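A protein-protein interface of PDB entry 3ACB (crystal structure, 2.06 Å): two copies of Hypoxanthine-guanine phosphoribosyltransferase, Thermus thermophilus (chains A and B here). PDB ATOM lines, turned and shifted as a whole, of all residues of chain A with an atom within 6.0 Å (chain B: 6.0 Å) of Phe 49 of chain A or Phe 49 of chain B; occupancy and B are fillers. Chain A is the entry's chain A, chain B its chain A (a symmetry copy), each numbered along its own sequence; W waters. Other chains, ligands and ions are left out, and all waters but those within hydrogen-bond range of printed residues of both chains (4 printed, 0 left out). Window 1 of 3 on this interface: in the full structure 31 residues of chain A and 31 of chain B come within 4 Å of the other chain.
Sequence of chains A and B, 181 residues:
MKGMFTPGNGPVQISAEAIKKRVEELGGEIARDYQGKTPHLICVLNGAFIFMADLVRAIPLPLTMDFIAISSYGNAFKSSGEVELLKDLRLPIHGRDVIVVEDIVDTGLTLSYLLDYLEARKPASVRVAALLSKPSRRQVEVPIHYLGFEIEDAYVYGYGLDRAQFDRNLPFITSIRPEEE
The backbone NH (N) of Phe 49 of chain A is in hydrogen-bond range of the side-chain sulfur (SG) of Cys 43 of chain A (3.7 Å). O of Gly 160 of chain A lies within hydrogen-bond range of NH1 of Arg 168 of chain A (2.8 Å). The backbone NH (N) of Phe 49 of chain B sits at hydrogen-bond distance from the side-chain sulfur (SG) of Cys 43 of chain B. O of Gly 160 of chain B is in hydrogen-bond range of NH1 of Arg 168 of chain B (2.8 Å).
Among the printed residues, pairs that only touch across the chains: Leu 45 of chain A with Leu 45 of chain B, Asn 46 of chain A with Phe 67 of chain B, Phe 49 of chain A with Phe 49 of chain B, Phe 49 of chain A with Met 52 of chain B, Phe 49 of chain A with Ala 53 of chain B, Phe 49 of chain A with Met 65 of chain B, Phe 49 of chain A with Phe 67 of chain B, Met 52 of chain A with Phe 49 of chain B, Ala 53 of chain A with Phe 49 of chain B, Ala 53 of chain A with Ala 53 of chain B, Met 65 of chain A with Phe 49 of chain B, Met 65 of chain A with Arg 168 of chain B, Phe 67 of chain A with Asn 46 of chain B, Phe 67 of chain A with Phe 49 of chain B and Arg 168 of chain A with Met 65 of chain B.
Of chain B, only Phe 49, Met 52, Ala 53, Met 65 and Phe 67 come within 4 Å of Phe 49 of chain A. Of chain A, only Phe 49, Met 52, Ala 53, Met 65 and Phe 67 come within 4 Å of Phe 49 of chain B. Of the printed residues of chain B, Met 52 of chain A touches Phe 49. Of the printed residues of chain B, Arg 168 of chain A touches Met 65 (3.6 Å). Printed residues of chain A within 4 Å of Ala 53 of chain B: Phe 49 (3.6 Å) and Ala 53 (3.6 Å). The nearest residue of chain A that does not touch Phe 49 of chain B is Val 56 of chain A (4.4 Å).
Printed residues of chain A that touch a printed residue of chain B: Leu 45, Asn 46, Phe 49, Met 52, Ala 53, Met 65, Phe 67 and Arg 168. Of the 17 printed residues of chain B, 8 touch a printed residue of chain A. Along chain B the printed residues that touch a printed residue of chain A span positions 45 to 168. Among the printed residues, no Asp or Glu carboxylate lies within 4 Å of a Lys or Arg side-chain nitrogen of the other chain.
Leu 45 of chain B touches its own counterpart, Leu 45 of chain A. Phe 49 of chain A touches its own counterpart, Phe 49 of chain B. Phe 49 of chain A touches Met 65 of chain B, and with the chains exchanged Met 65 of chain A touches Phe 49 of chain B. Met 65 of chain A touches Arg 168 of chain B, and with the chains exchanged Arg 168 of chain A touches Met 65 of chain B. Positions printed for both chains: 43, 44, 45, 46, 47, 48, 49, 50, 51, 52, 53, 54, 56, 65, 67, 160 and 168.
Water W3 lies within hydrogen-bond range of O of Met 65 of chain B (2.8 Å), OD1 of Asn 46 of chain A (2.9 Å) and NH2 of Arg 168 of chain A (3.4 Å). Water W4 lies within hydrogen-bond range of the backbone carbonyl oxygen of Met 65 of chain A (2.8 Å), the side-chain amide oxygen of Asn 46 of chain B (2.9 Å) and the guanidinium group of Arg 168 of chain B (3.4 Å). Water W2 bridges the backbone NH of Met 65 of chain B (3.0 Å) and the guanidinium group of Arg 168 of chain A (3.0 Å). Water W1 lies within hydrogen-bond range of N of Met 65 of chain A and NE of Arg 168 of chain B.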
ATOM      1  N   CYS A  43      -1.913 -12.175 -32.077  1.00  0.00           N
ATOM      2  CA  CYS A  43      -1.820 -13.382 -31.275  1.00  0.00           C
ATOM      3  C   CYS A  43      -2.563 -14.553 -31.923  1.00  0.00           C
ATOM      4  O   CYS A  43      -3.751 -14.448 -32.244  1.00  0.00           O
ATOM      5  CB  CYS A  43      -2.400 -13.115 -29.883  1.00  0.00           C
ATOM      6  SG  CYS A  43      -2.594 -14.590 -28.837  1.00  0.00           S
ATOM      7  N   VAL A  44      -1.859 -15.665 -32.117  1.00  0.00           N
ATOM      8  CA  VAL A  44      -2.468 -16.854 -32.697  1.00  0.00           C
ATOM      9  C   VAL A  44      -3.121 -17.667 -31.578  1.00  0.00           C
ATOM     10  O   VAL A  44      -2.434 -18.325 -30.789  1.00  0.00           O
ATOM     11  CB  VAL A  44      -1.408 -17.725 -33.416  1.00  0.00           C
ATOM     12  CG1 VAL A  44      -2.056 -18.987 -33.979  1.00  0.00           C
ATOM     13  CG2 VAL A  44      -0.755 -16.923 -34.531  1.00  0.00           C
ATOM     14  N   LEU A  45      -4.449 -17.609 -31.504  1.00  0.00           N
ATOM     15  CA  LEU A  45      -5.208 -18.340 -30.487  1.00  0.00           C
ATOM     16  C   LEU A  45      -5.294 -19.827 -30.827  1.00  0.00           C
ATOM     17  O   LEU A  45      -5.221 -20.190 -31.998  1.00  0.00           O
ATOM     18  CB  LEU A  45      -6.625 -17.772 -30.376  1.00  0.00           C
ATOM     19  CG  LEU A  45      -6.765 -16.365 -29.795  1.00  0.00           C
ATOM     20  CD1 LEU A  45      -8.219 -15.919 -29.883  1.00  0.00           C
ATOM     21  CD2 LEU A  45      -6.285 -16.366 -28.345  1.00  0.00           C
ATOM     22  N   ASN A  46      -5.451 -20.687 -29.821  1.00  0.00           N
ATOM     23  CA  ASN A  46      -5.541 -20.293 -28.411  1.00  0.00           C
ATOM     24  C   ASN A  46      -4.180 -20.344 -27.714  1.00  0.00           C
ATOM     25  O   ASN A  46      -3.921 -19.586 -26.778  1.00  0.00           O
ATOM     26  CB  ASN A  46      -6.472 -21.247 -27.649  1.00  0.00           C
ATOM     27  CG  ASN A  46      -7.923 -21.151 -28.092  1.00  0.00           C
ATOM     28  OD1 ASN A  46      -8.754 -21.969 -27.685  1.00  0.00           O
ATOM     29  ND2 ASN A  46      -8.236 -20.153 -28.910  1.00  0.00           N
ATOM     30  N   GLY A  47      -3.327 -21.250 -28.183  1.00  0.00           N
ATOM     31  CA  GLY A  47      -2.019 -21.470 -27.590  1.00  0.00           C
ATOM     32  C   GLY A  47      -1.067 -20.349 -27.222  1.00  0.00           C
ATOM     33  O   GLY A  47      -0.321 -20.481 -26.251  1.00  0.00           O
ATOM     34  N   ALA A  48      -1.073 -19.251 -27.967  1.00  0.00           N
ATOM     35  CA  ALA A  48      -0.137 -18.168 -27.689  1.00  0.00           C
ATOM     36  C   ALA A  48      -0.633 -17.060 -26.776  1.00  0.00           C
ATOM     37  O   ALA A  48       0.109 -16.124 -26.502  1.00  0.00           O
ATOM     38  CB  ALA A  48       0.340 -17.559 -29.010  1.00  0.00           C
ATOM     39  N   PHE A  49      -1.861 -17.167 -26.276  1.00  0.00           N
ATOM     40  CA  PHE A  49      -2.407 -16.093 -25.454  1.00  0.00           C
ATOM     41  C   PHE A  49      -1.634 -15.710 -24.190  1.00  0.00           C
ATOM     42  O   PHE A  49      -1.604 -14.534 -23.824  1.00  0.00           O
ATOM     43  CB  PHE A  49      -3.890 -16.374 -25.144  1.00  0.00           C
ATOM     44  CG  PHE A  49      -4.145 -17.020 -23.814  1.00  0.00           C
ATOM     45  CD1 PHE A  49      -4.441 -16.243 -22.695  1.00  0.00           C
ATOM     46  CD2 PHE A  49      -4.171 -18.406 -23.692  1.00  0.00           C
ATOM     47  CE1 PHE A  49      -4.766 -16.839 -21.478  1.00  0.00           C
ATOM     48  CE2 PHE A  49      -4.496 -19.014 -22.476  1.00  0.00           C
ATOM     49  CZ  PHE A  49      -4.795 -18.230 -21.369  1.00  0.00           C
ATOM     50  N   ILE A  50      -1.002 -16.668 -23.521  1.00  0.00           N
ATOM     51  CA  ILE A  50      -0.245 -16.325 -22.316  1.00  0.00           C
ATOM     52  C   ILE A  50       1.090 -15.704 -22.734  1.00  0.00           C
ATOM     53  O   ILE A  50       1.536 -14.715 -22.156  1.00  0.00           O
ATOM     54  CB  ILE A  50      -0.011 -17.564 -21.419  1.00  0.00           C
ATOM     55  CG1 ILE A  50      -1.367 -18.154 -21.006  1.00  0.00           C
ATOM     56  CG2 ILE A  50       0.812 -17.169 -20.182  1.00  0.00           C
ATOM     57  CD1 ILE A  50      -1.300 -19.203 -19.900  1.00  0.00           C
ATOM     58  N   PHE A  51       1.720 -16.281 -23.754  1.00  0.00           N
ATOM     59  CA  PHE A  51       2.976 -15.754 -24.273  1.00  0.00           C
ATOM     60  C   PHE A  51       2.717 -14.304 -24.703  1.00  0.00           C
ATOM     61  O   PHE A  51       3.506 -13.403 -24.415  1.00  0.00           O
ATOM     62  CB  PHE A  51       3.427 -16.609 -25.469  1.00  0.00           C
ATOM     63  CG  PHE A  51       4.632 -16.071 -26.206  1.00  0.00           C
ATOM     64  CD1 PHE A  51       5.732 -15.574 -25.519  1.00  0.00           C
ATOM     65  CD2 PHE A  51       4.679 -16.113 -27.598  1.00  0.00           C
ATOM     66  CE1 PHE A  51       6.869 -15.131 -26.210  1.00  0.00           C
ATOM     67  CE2 PHE A  51       5.808 -15.675 -28.301  1.00  0.00           C
ATOM     68  CZ  PHE A  51       6.905 -15.182 -27.604  1.00  0.00           C
ATOM     69  N   MET A  52       1.591 -14.090 -25.378  1.00  0.00           N
ATOM     70  CA  MET A  52       1.208 -12.760 -25.847  1.00  0.00           C
ATOM     71  C   MET A  52       1.067 -11.778 -24.678  1.00  0.00           C
ATOM     72  O   MET A  52       1.581 -10.659 -24.723  1.00  0.00           O
ATOM     73  CB  MET A  52      -0.121 -12.848 -26.611  1.00  0.00           C
ATOM     74  CG  MET A  52      -0.673 -11.514 -27.088  1.00  0.00           C
ATOM     75  SD  MET A  52       0.163 -10.886 -28.548  1.00  0.00           S
ATOM     76  CE  MET A  52      -0.943  -9.531 -29.033  1.00  0.00           C
ATOM     77  N   ALA A  53       0.364 -12.205 -23.634  1.00  0.00           N
ATOM     78  CA  ALA A  53       0.137 -11.367 -22.460  1.00  0.00           C
ATOM     79  C   ALA A  53       1.436 -10.932 -21.778  1.00  0.00           C
ATOM     80  O   ALA A  53       1.588  -9.768 -21.396  1.00  0.00           O
ATOM     81  CB  ALA A  53      -0.753 -12.105 -21.465  1.00  0.00           C
ATOM     82  N   ASP A  54       2.371 -11.861 -21.619  1.00  0.00           N
ATOM     83  CA  ASP A  54       3.634 -11.524 -20.979  1.00  0.00           C
ATOM     84  C   ASP A  54       4.538 -10.718 -21.899  1.00  0.00           C
ATOM     85  O   ASP A  54       5.216  -9.794 -21.456  1.00  0.00           O
ATOM     86  CB  ASP A  54       4.356 -12.791 -20.513  1.00  0.00           C
ATOM     87  CG  ASP A  54       3.612 -13.507 -19.404  1.00  0.00           C
ATOM     88  OD1 ASP A  54       2.630 -12.930 -18.879  1.00  0.00           O
ATOM     89  OD2 ASP A  54       4.006 -14.642 -19.053  1.00  0.00           O
ATOM     90  N   VAL A  56       3.705  -8.596 -24.510  1.00  0.00           N
ATOM     91  CA  VAL A  56       3.301  -7.209 -24.725  1.00  0.00           C
ATOM     92  C   VAL A  56       3.672  -6.318 -23.545  1.00  0.00           C
ATOM     93  O   VAL A  56       4.043  -5.154 -23.719  1.00  0.00           O
ATOM     94  CB  VAL A  56       1.791  -7.087 -25.005  1.00  0.00           C
ATOM     95  CG1 VAL A  56       1.442  -7.852 -26.279  1.00  0.00           C
ATOM     96  CG2 VAL A  56       0.989  -7.599 -23.820  1.00  0.00           C
ATOM     97  N   MET A  65      -3.119  -4.481 -31.137  1.00  0.00           N
ATOM     98  CA  MET A  65      -3.091  -5.927 -31.239  1.00  0.00           C
ATOM     99  C   MET A  65      -4.395  -6.505 -31.746  1.00  0.00           C
ATOM    100  O   MET A  65      -5.412  -5.825 -31.799  1.00  0.00           O
ATOM    101  CB  MET A  65      -2.704  -6.564 -29.889  1.00  0.00           C
ATOM    102  CG  MET A  65      -3.152  -5.816 -28.642  1.00  0.00           C
ATOM    103  SD  MET A  65      -2.529  -6.540 -27.077  1.00  0.00           S
ATOM    104  CE  MET A  65      -1.247  -5.390 -26.628  1.00  0.00           C
ATOM    105  N   PHE A  67      -6.406 -10.684 -32.530  1.00  0.00           N
ATOM    106  CA  PHE A  67      -6.381 -12.109 -32.280  1.00  0.00           C
ATOM    107  C   PHE A  67      -6.945 -12.859 -33.466  1.00  0.00           C
ATOM    108  O   PHE A  67      -7.943 -12.448 -34.060  1.00  0.00           O
ATOM    109  CB  PHE A  67      -7.203 -12.416 -31.034  1.00  0.00           C
ATOM    110  CG  PHE A  67      -6.658 -11.788 -29.790  1.00  0.00           C
ATOM    111  CD1 PHE A  67      -5.817 -12.508 -28.941  1.00  0.00           C
ATOM    112  CD2 PHE A  67      -6.962 -10.467 -29.473  1.00  0.00           C
ATOM    113  CE1 PHE A  67      -5.289 -11.922 -27.795  1.00  0.00           C
ATOM    114  CE2 PHE A  67      -6.439  -9.871 -28.331  1.00  0.00           C
ATOM    115  CZ  PHE A  67      -5.599 -10.602 -27.488  1.00  0.00           C
ATOM    116  N   GLY A 160      -0.133 -21.979 -21.754  1.00  0.00           N
ATOM    117  CA  GLY A 160      -1.005 -21.686 -22.876  1.00  0.00           C
ATOM    118  C   GLY A 160      -1.253 -22.870 -23.798  1.00  0.00           C
ATOM    119  O   GLY A 160      -2.325 -22.970 -24.395  1.00  0.00           O
ATOM    120  N   ARG A 168      -3.407 -25.818 -19.872  1.00  0.00           N
ATOM    121  CA  ARG A 168      -2.934 -24.573 -20.470  1.00  0.00           C
ATOM    122  C   ARG A 168      -2.537 -23.628 -19.336  1.00  0.00           C
ATOM    123  O   ARG A 168      -1.780 -22.676 -19.546  1.00  0.00           O
ATOM    124  CB  ARG A 168      -4.032 -23.876 -21.283  1.00  0.00           C
ATOM    125  CG  ARG A 168      -4.471 -24.545 -22.573  1.00  0.00           C
ATOM    126  CD  ARG A 168      -5.518 -23.656 -23.257  1.00  0.00           C
ATOM    127  NE  ARG A 168      -6.209 -24.316 -24.367  1.00  0.00           N
ATOM    128  CZ  ARG A 168      -5.677 -24.530 -25.565  1.00  0.00           C
ATOM    129  NH1 ARG A 168      -4.435 -24.135 -25.824  1.00  0.00           N
ATOM    130  NH2 ARG A 168      -6.389 -25.144 -26.504  1.00  0.00           N
ATOM    131  N   CYS B  43     -12.785 -16.688 -21.458  1.00  0.00           N
ATOM    132  CA  CYS B  43     -12.217 -15.353 -21.529  1.00  0.00           C
ATOM    133  C   CYS B  43     -12.965 -14.469 -22.531  1.00  0.00           C
ATOM    134  O   CYS B  43     -13.125 -14.833 -23.700  1.00  0.00           O
ATOM    135  CB  CYS B  43     -10.743 -15.448 -21.932  1.00  0.00           C
ATOM    136  SG  CYS B  43      -9.948 -13.858 -22.315  1.00  0.00           S
ATOM    137  N   VAL B  44     -13.425 -13.310 -22.067  1.00  0.00           N
ATOM    138  CA  VAL B  44     -14.126 -12.374 -22.935  1.00  0.00           C
ATOM    139  C   VAL B  44     -13.094 -11.488 -23.635  1.00  0.00           C
ATOM    140  O   VAL B  44     -12.513 -10.586 -23.022  1.00  0.00           O
ATOM    141  CB  VAL B  44     -15.100 -11.486 -22.120  1.00  0.00           C
ATOM    142  CG1 VAL B  44     -15.790 -10.481 -23.038  1.00  0.00           C
ATOM    143  CG2 VAL B  44     -16.129 -12.360 -21.421  1.00  0.00           C
ATOM    144  N   LEU B  45     -12.859 -11.756 -24.917  1.00  0.00           N
ATOM    145  CA  LEU B  45     -11.900 -10.986 -25.714  1.00  0.00           C
ATOM    146  C   LEU B  45     -12.477  -9.626 -26.106  1.00  0.00           C
ATOM    147  O   LEU B  45     -13.693  -9.483 -26.200  1.00  0.00           O
ATOM    148  CB  LEU B  45     -11.533 -11.756 -26.986  1.00  0.00           C
ATOM    149  CG  LEU B  45     -10.708 -13.031 -26.809  1.00  0.00           C
ATOM    150  CD1 LEU B  45     -10.551 -13.727 -28.156  1.00  0.00           C
ATOM    151  CD2 LEU B  45      -9.344 -12.676 -26.220  1.00  0.00           C
ATOM    152  N   ASN B  46     -11.621  -8.632 -26.340  1.00  0.00           N
ATOM    153  CA  ASN B  46     -10.164  -8.763 -26.237  1.00  0.00           C
ATOM    154  C   ASN B  46      -9.646  -8.351 -24.858  1.00  0.00           C
ATOM    155  O   ASN B  46      -8.631  -8.863 -24.385  1.00  0.00           O
ATOM    156  CB  ASN B  46      -9.473  -7.855 -27.265  1.00  0.00           C
ATOM    157  CG  ASN B  46      -9.724  -8.278 -28.704  1.00  0.00           C
ATOM    158  OD1 ASN B  46      -9.370  -7.553 -29.639  1.00  0.00           O
ATOM    159  ND2 ASN B  46     -10.319  -9.451 -28.890  1.00  0.00           N
ATOM    160  N   GLY B  47     -10.357  -7.418 -24.232  1.00  0.00           N
ATOM    161  CA  GLY B  47      -9.966  -6.870 -22.945  1.00  0.00           C
ATOM    162  C   GLY B  47      -9.524  -7.722 -21.772  1.00  0.00           C
ATOM    163  O   GLY B  47      -8.681  -7.285 -20.987  1.00  0.00           O
ATOM    164  N   ALA B  48     -10.065  -8.926 -21.631  1.00  0.00           N
ATOM    165  CA  ALA B  48      -9.716  -9.762 -20.490  1.00  0.00           C
ATOM    166  C   ALA B  48      -8.577 -10.746 -20.690  1.00  0.00           C
ATOM    167  O   ALA B  48      -8.234 -11.474 -19.765  1.00  0.00           O
ATOM    168  CB  ALA B  48     -10.960 -10.519 -20.017  1.00  0.00           C
ATOM    169  N   PHE B  49      -7.965 -10.758 -21.872  1.00  0.00           N
ATOM    170  CA  PHE B  49      -6.914 -11.734 -22.136  1.00  0.00           C
ATOM    171  C   PHE B  49      -5.701 -11.735 -21.204  1.00  0.00           C
ATOM    172  O   PHE B  49      -5.145 -12.798 -20.923  1.00  0.00           O
ATOM    173  CB  PHE B  49      -6.488 -11.657 -23.615  1.00  0.00           C
ATOM    174  CG  PHE B  49      -5.267 -10.825 -23.878  1.00  0.00           C
ATOM    175  CD1 PHE B  49      -4.007 -11.416 -23.929  1.00  0.00           C
ATOM    176  CD2 PHE B  49      -5.381  -9.466 -24.153  1.00  0.00           C
ATOM    177  CE1 PHE B  49      -2.880 -10.666 -24.259  1.00  0.00           C
ATOM    178  CE2 PHE B  49      -4.257  -8.704 -24.486  1.00  0.00           C
ATOM    179  CZ  PHE B  49      -3.006  -9.305 -24.540  1.00  0.00           C
ATOM    180  N   ILE B  50      -5.281 -10.575 -20.711  1.00  0.00           N
ATOM    181  CA  ILE B  50      -4.132 -10.551 -19.807  1.00  0.00           C
ATOM    182  C   ILE B  50      -4.589 -11.003 -18.417  1.00  0.00           C
ATOM    183  O   ILE B  50      -3.905 -11.774 -17.748  1.00  0.00           O
ATOM    184  CB  ILE B  50      -3.491  -9.144 -19.737  1.00  0.00           C
ATOM    185  CG1 ILE B  50      -3.032  -8.726 -21.142  1.00  0.00           C
ATOM    186  CG2 ILE B  50      -2.307  -9.152 -18.755  1.00  0.00           C
ATOM    187  CD1 ILE B  50      -2.136  -7.491 -21.182  1.00  0.00           C
ATOM    188  N   PHE B  51      -5.757 -10.530 -17.994  1.00  0.00           N
ATOM    189  CA  PHE B  51      -6.319 -10.923 -16.707  1.00  0.00           C
ATOM    190  C   PHE B  51      -6.463 -12.451 -16.722  1.00  0.00           C
ATOM    191  O   PHE B  51      -6.119 -13.133 -15.758  1.00  0.00           O
ATOM    192  CB  PHE B  51      -7.687 -10.245 -16.526  1.00  0.00           C
ATOM    193  CG  PHE B  51      -8.455 -10.698 -15.306  1.00  0.00           C
ATOM    194  CD1 PHE B  51      -7.825 -10.863 -14.078  1.00  0.00           C
ATOM    195  CD2 PHE B  51      -9.830 -10.912 -15.382  1.00  0.00           C
ATOM    196  CE1 PHE B  51      -8.557 -11.227 -12.939  1.00  0.00           C
ATOM    197  CE2 PHE B  51     -10.574 -11.276 -14.251  1.00  0.00           C
ATOM    198  CZ  PHE B  51      -9.934 -11.434 -13.028  1.00  0.00           C
ATOM    199  N   MET B  52      -6.958 -12.977 -17.840  1.00  0.00           N
ATOM    200  CA  MET B  52      -7.147 -14.417 -18.003  1.00  0.00           C
ATOM    201  C   MET B  52      -5.819 -15.170 -17.860  1.00  0.00           C
ATOM    202  O   MET B  52      -5.732 -16.174 -17.150  1.00  0.00           O
ATOM    203  CB  MET B  52      -7.756 -14.701 -19.382  1.00  0.00           C
ATOM    204  CG  MET B  52      -7.932 -16.176 -19.711  1.00  0.00           C
ATOM    205  SD  MET B  52      -9.351 -16.915 -18.895  1.00  0.00           S
ATOM    206  CE  MET B  52      -9.467 -18.506 -19.761  1.00  0.00           C
ATOM    207  N   ALA B  53      -4.789 -14.680 -18.543  1.00  0.00           N
ATOM    208  CA  ALA B  53      -3.472 -15.308 -18.510  1.00  0.00           C
ATOM    209  C   ALA B  53      -2.880 -15.380 -17.101  1.00  0.00           C
ATOM    210  O   ALA B  53      -2.325 -16.407 -16.702  1.00  0.00           O
ATOM    211  CB  ALA B  53      -2.522 -14.559 -19.439  1.00  0.00           C
ATOM    212  N   ASP B  54      -2.989 -14.291 -16.348  1.00  0.00           N
ATOM    213  CA  ASP B  54      -2.451 -14.282 -14.996  1.00  0.00           C
ATOM    214  C   ASP B  54      -3.318 -15.081 -14.035  1.00  0.00           C
ATOM    215  O   ASP B  54      -2.804 -15.775 -13.160  1.00  0.00           O
ATOM    216  CB  ASP B  54      -2.294 -12.846 -14.489  1.00  0.00           C
ATOM    217  CG  ASP B  54      -1.244 -12.070 -15.261  1.00  0.00           C
ATOM    218  OD1 ASP B  54      -0.520 -12.697 -16.071  1.00  0.00           O
ATOM    219  OD2 ASP B  54      -1.140 -10.840 -15.062  1.00  0.00           O
ATOM    220  N   VAL B  56      -5.416 -17.766 -14.665  1.00  0.00           N
ATOM    221  CA  VAL B  56      -5.344 -19.218 -14.817  1.00  0.00           C
ATOM    222  C   VAL B  56      -4.079 -19.794 -14.189  1.00  0.00           C
ATOM    223  O   VAL B  56      -4.094 -20.889 -13.621  1.00  0.00           O
ATOM    224  CB  VAL B  56      -5.424 -19.646 -16.295  1.00  0.00           C
ATOM    225  CG1 VAL B  56      -6.760 -19.206 -16.885  1.00  0.00           C
ATOM    226  CG2 VAL B  56      -4.258 -19.064 -17.079  1.00  0.00           C
ATOM    227  N   MET B  65     -10.416 -24.157 -21.113  1.00  0.00           N
ATOM    228  CA  MET B  65     -10.765 -22.773 -21.366  1.00  0.00           C
ATOM    229  C   MET B  65     -11.210 -22.531 -22.793  1.00  0.00           C
ATOM    230  O   MET B  65     -11.029 -23.372 -23.665  1.00  0.00           O
ATOM    231  CB  MET B  65      -9.597 -21.837 -20.996  1.00  0.00           C
ATOM    232  CG  MET B  65      -8.198 -22.402 -21.191  1.00  0.00           C
ATOM    233  SD  MET B  65      -6.861 -21.300 -20.590  1.00  0.00           S
ATOM    234  CE  MET B  65      -6.374 -22.110 -19.082  1.00  0.00           C
ATOM    235  N   PHE B  67     -12.458 -18.980 -25.613  1.00  0.00           N
ATOM    236  CA  PHE B  67     -12.460 -17.550 -25.836  1.00  0.00           C
ATOM    237  C   PHE B  67     -13.684 -17.145 -26.626  1.00  0.00           C
ATOM    238  O   PHE B  67     -14.080 -17.824 -27.575  1.00  0.00           O
ATOM    239  CB  PHE B  67     -11.197 -17.158 -26.596  1.00  0.00           C
ATOM    240  CG  PHE B  67      -9.936 -17.440 -25.842  1.00  0.00           C
ATOM    241  CD1 PHE B  67      -9.325 -16.440 -25.085  1.00  0.00           C
ATOM    242  CD2 PHE B  67      -9.366 -18.709 -25.864  1.00  0.00           C
ATOM    243  CE1 PHE B  67      -8.163 -16.701 -24.364  1.00  0.00           C
ATOM    244  CE2 PHE B  67      -8.207 -18.981 -25.147  1.00  0.00           C
ATOM    245  CZ  PHE B  67      -7.603 -17.973 -24.392  1.00  0.00           C
ATOM    246  N   GLY B 160      -4.557  -4.957 -20.715  1.00  0.00           N
ATOM    247  CA  GLY B 160      -5.506  -5.600 -21.606  1.00  0.00           C
ATOM    248  C   GLY B 160      -6.581  -4.671 -22.147  1.00  0.00           C
ATOM    249  O   GLY B 160      -7.058  -4.869 -23.264  1.00  0.00           O
ATOM    250  N   ARG B 168      -2.993  -1.447 -24.489  1.00  0.00           N
ATOM    251  CA  ARG B 168      -3.420  -2.683 -23.840  1.00  0.00           C
ATOM    252  C   ARG B 168      -2.196  -3.316 -23.180  1.00  0.00           C
ATOM    253  O   ARG B 168      -2.326  -4.147 -22.277  1.00  0.00           O
ATOM    254  CB  ARG B 168      -3.971  -3.698 -24.849  1.00  0.00           C
ATOM    255  CG  ARG B 168      -5.297  -3.368 -25.512  1.00  0.00           C
ATOM    256  CD  ARG B 168      -5.695  -4.536 -26.424  1.00  0.00           C
ATOM    257  NE  ARG B 168      -6.814  -4.224 -27.316  1.00  0.00           N
ATOM    258  CZ  ARG B 168      -8.085  -4.153 -26.935  1.00  0.00           C
ATOM    259  NH1 ARG B 168      -8.413  -4.371 -25.666  1.00  0.00           N
ATOM    260  NH2 ARG B 168      -9.026  -3.856 -27.825  1.00  0.00           N
HETATM  261  O   HOH W   1      -5.466  -3.228 -29.820  1.00  0.00           O
HETATM  262  O   HOH W   2      -8.644 -25.521 -23.065  1.00  0.00           O
HETATM  263  O   HOH W   3      -9.591 -24.143 -25.943  1.00  0.00           O
HETATM  264  O   HOH W   4      -7.939  -5.264 -30.723  1.00  0.00           O
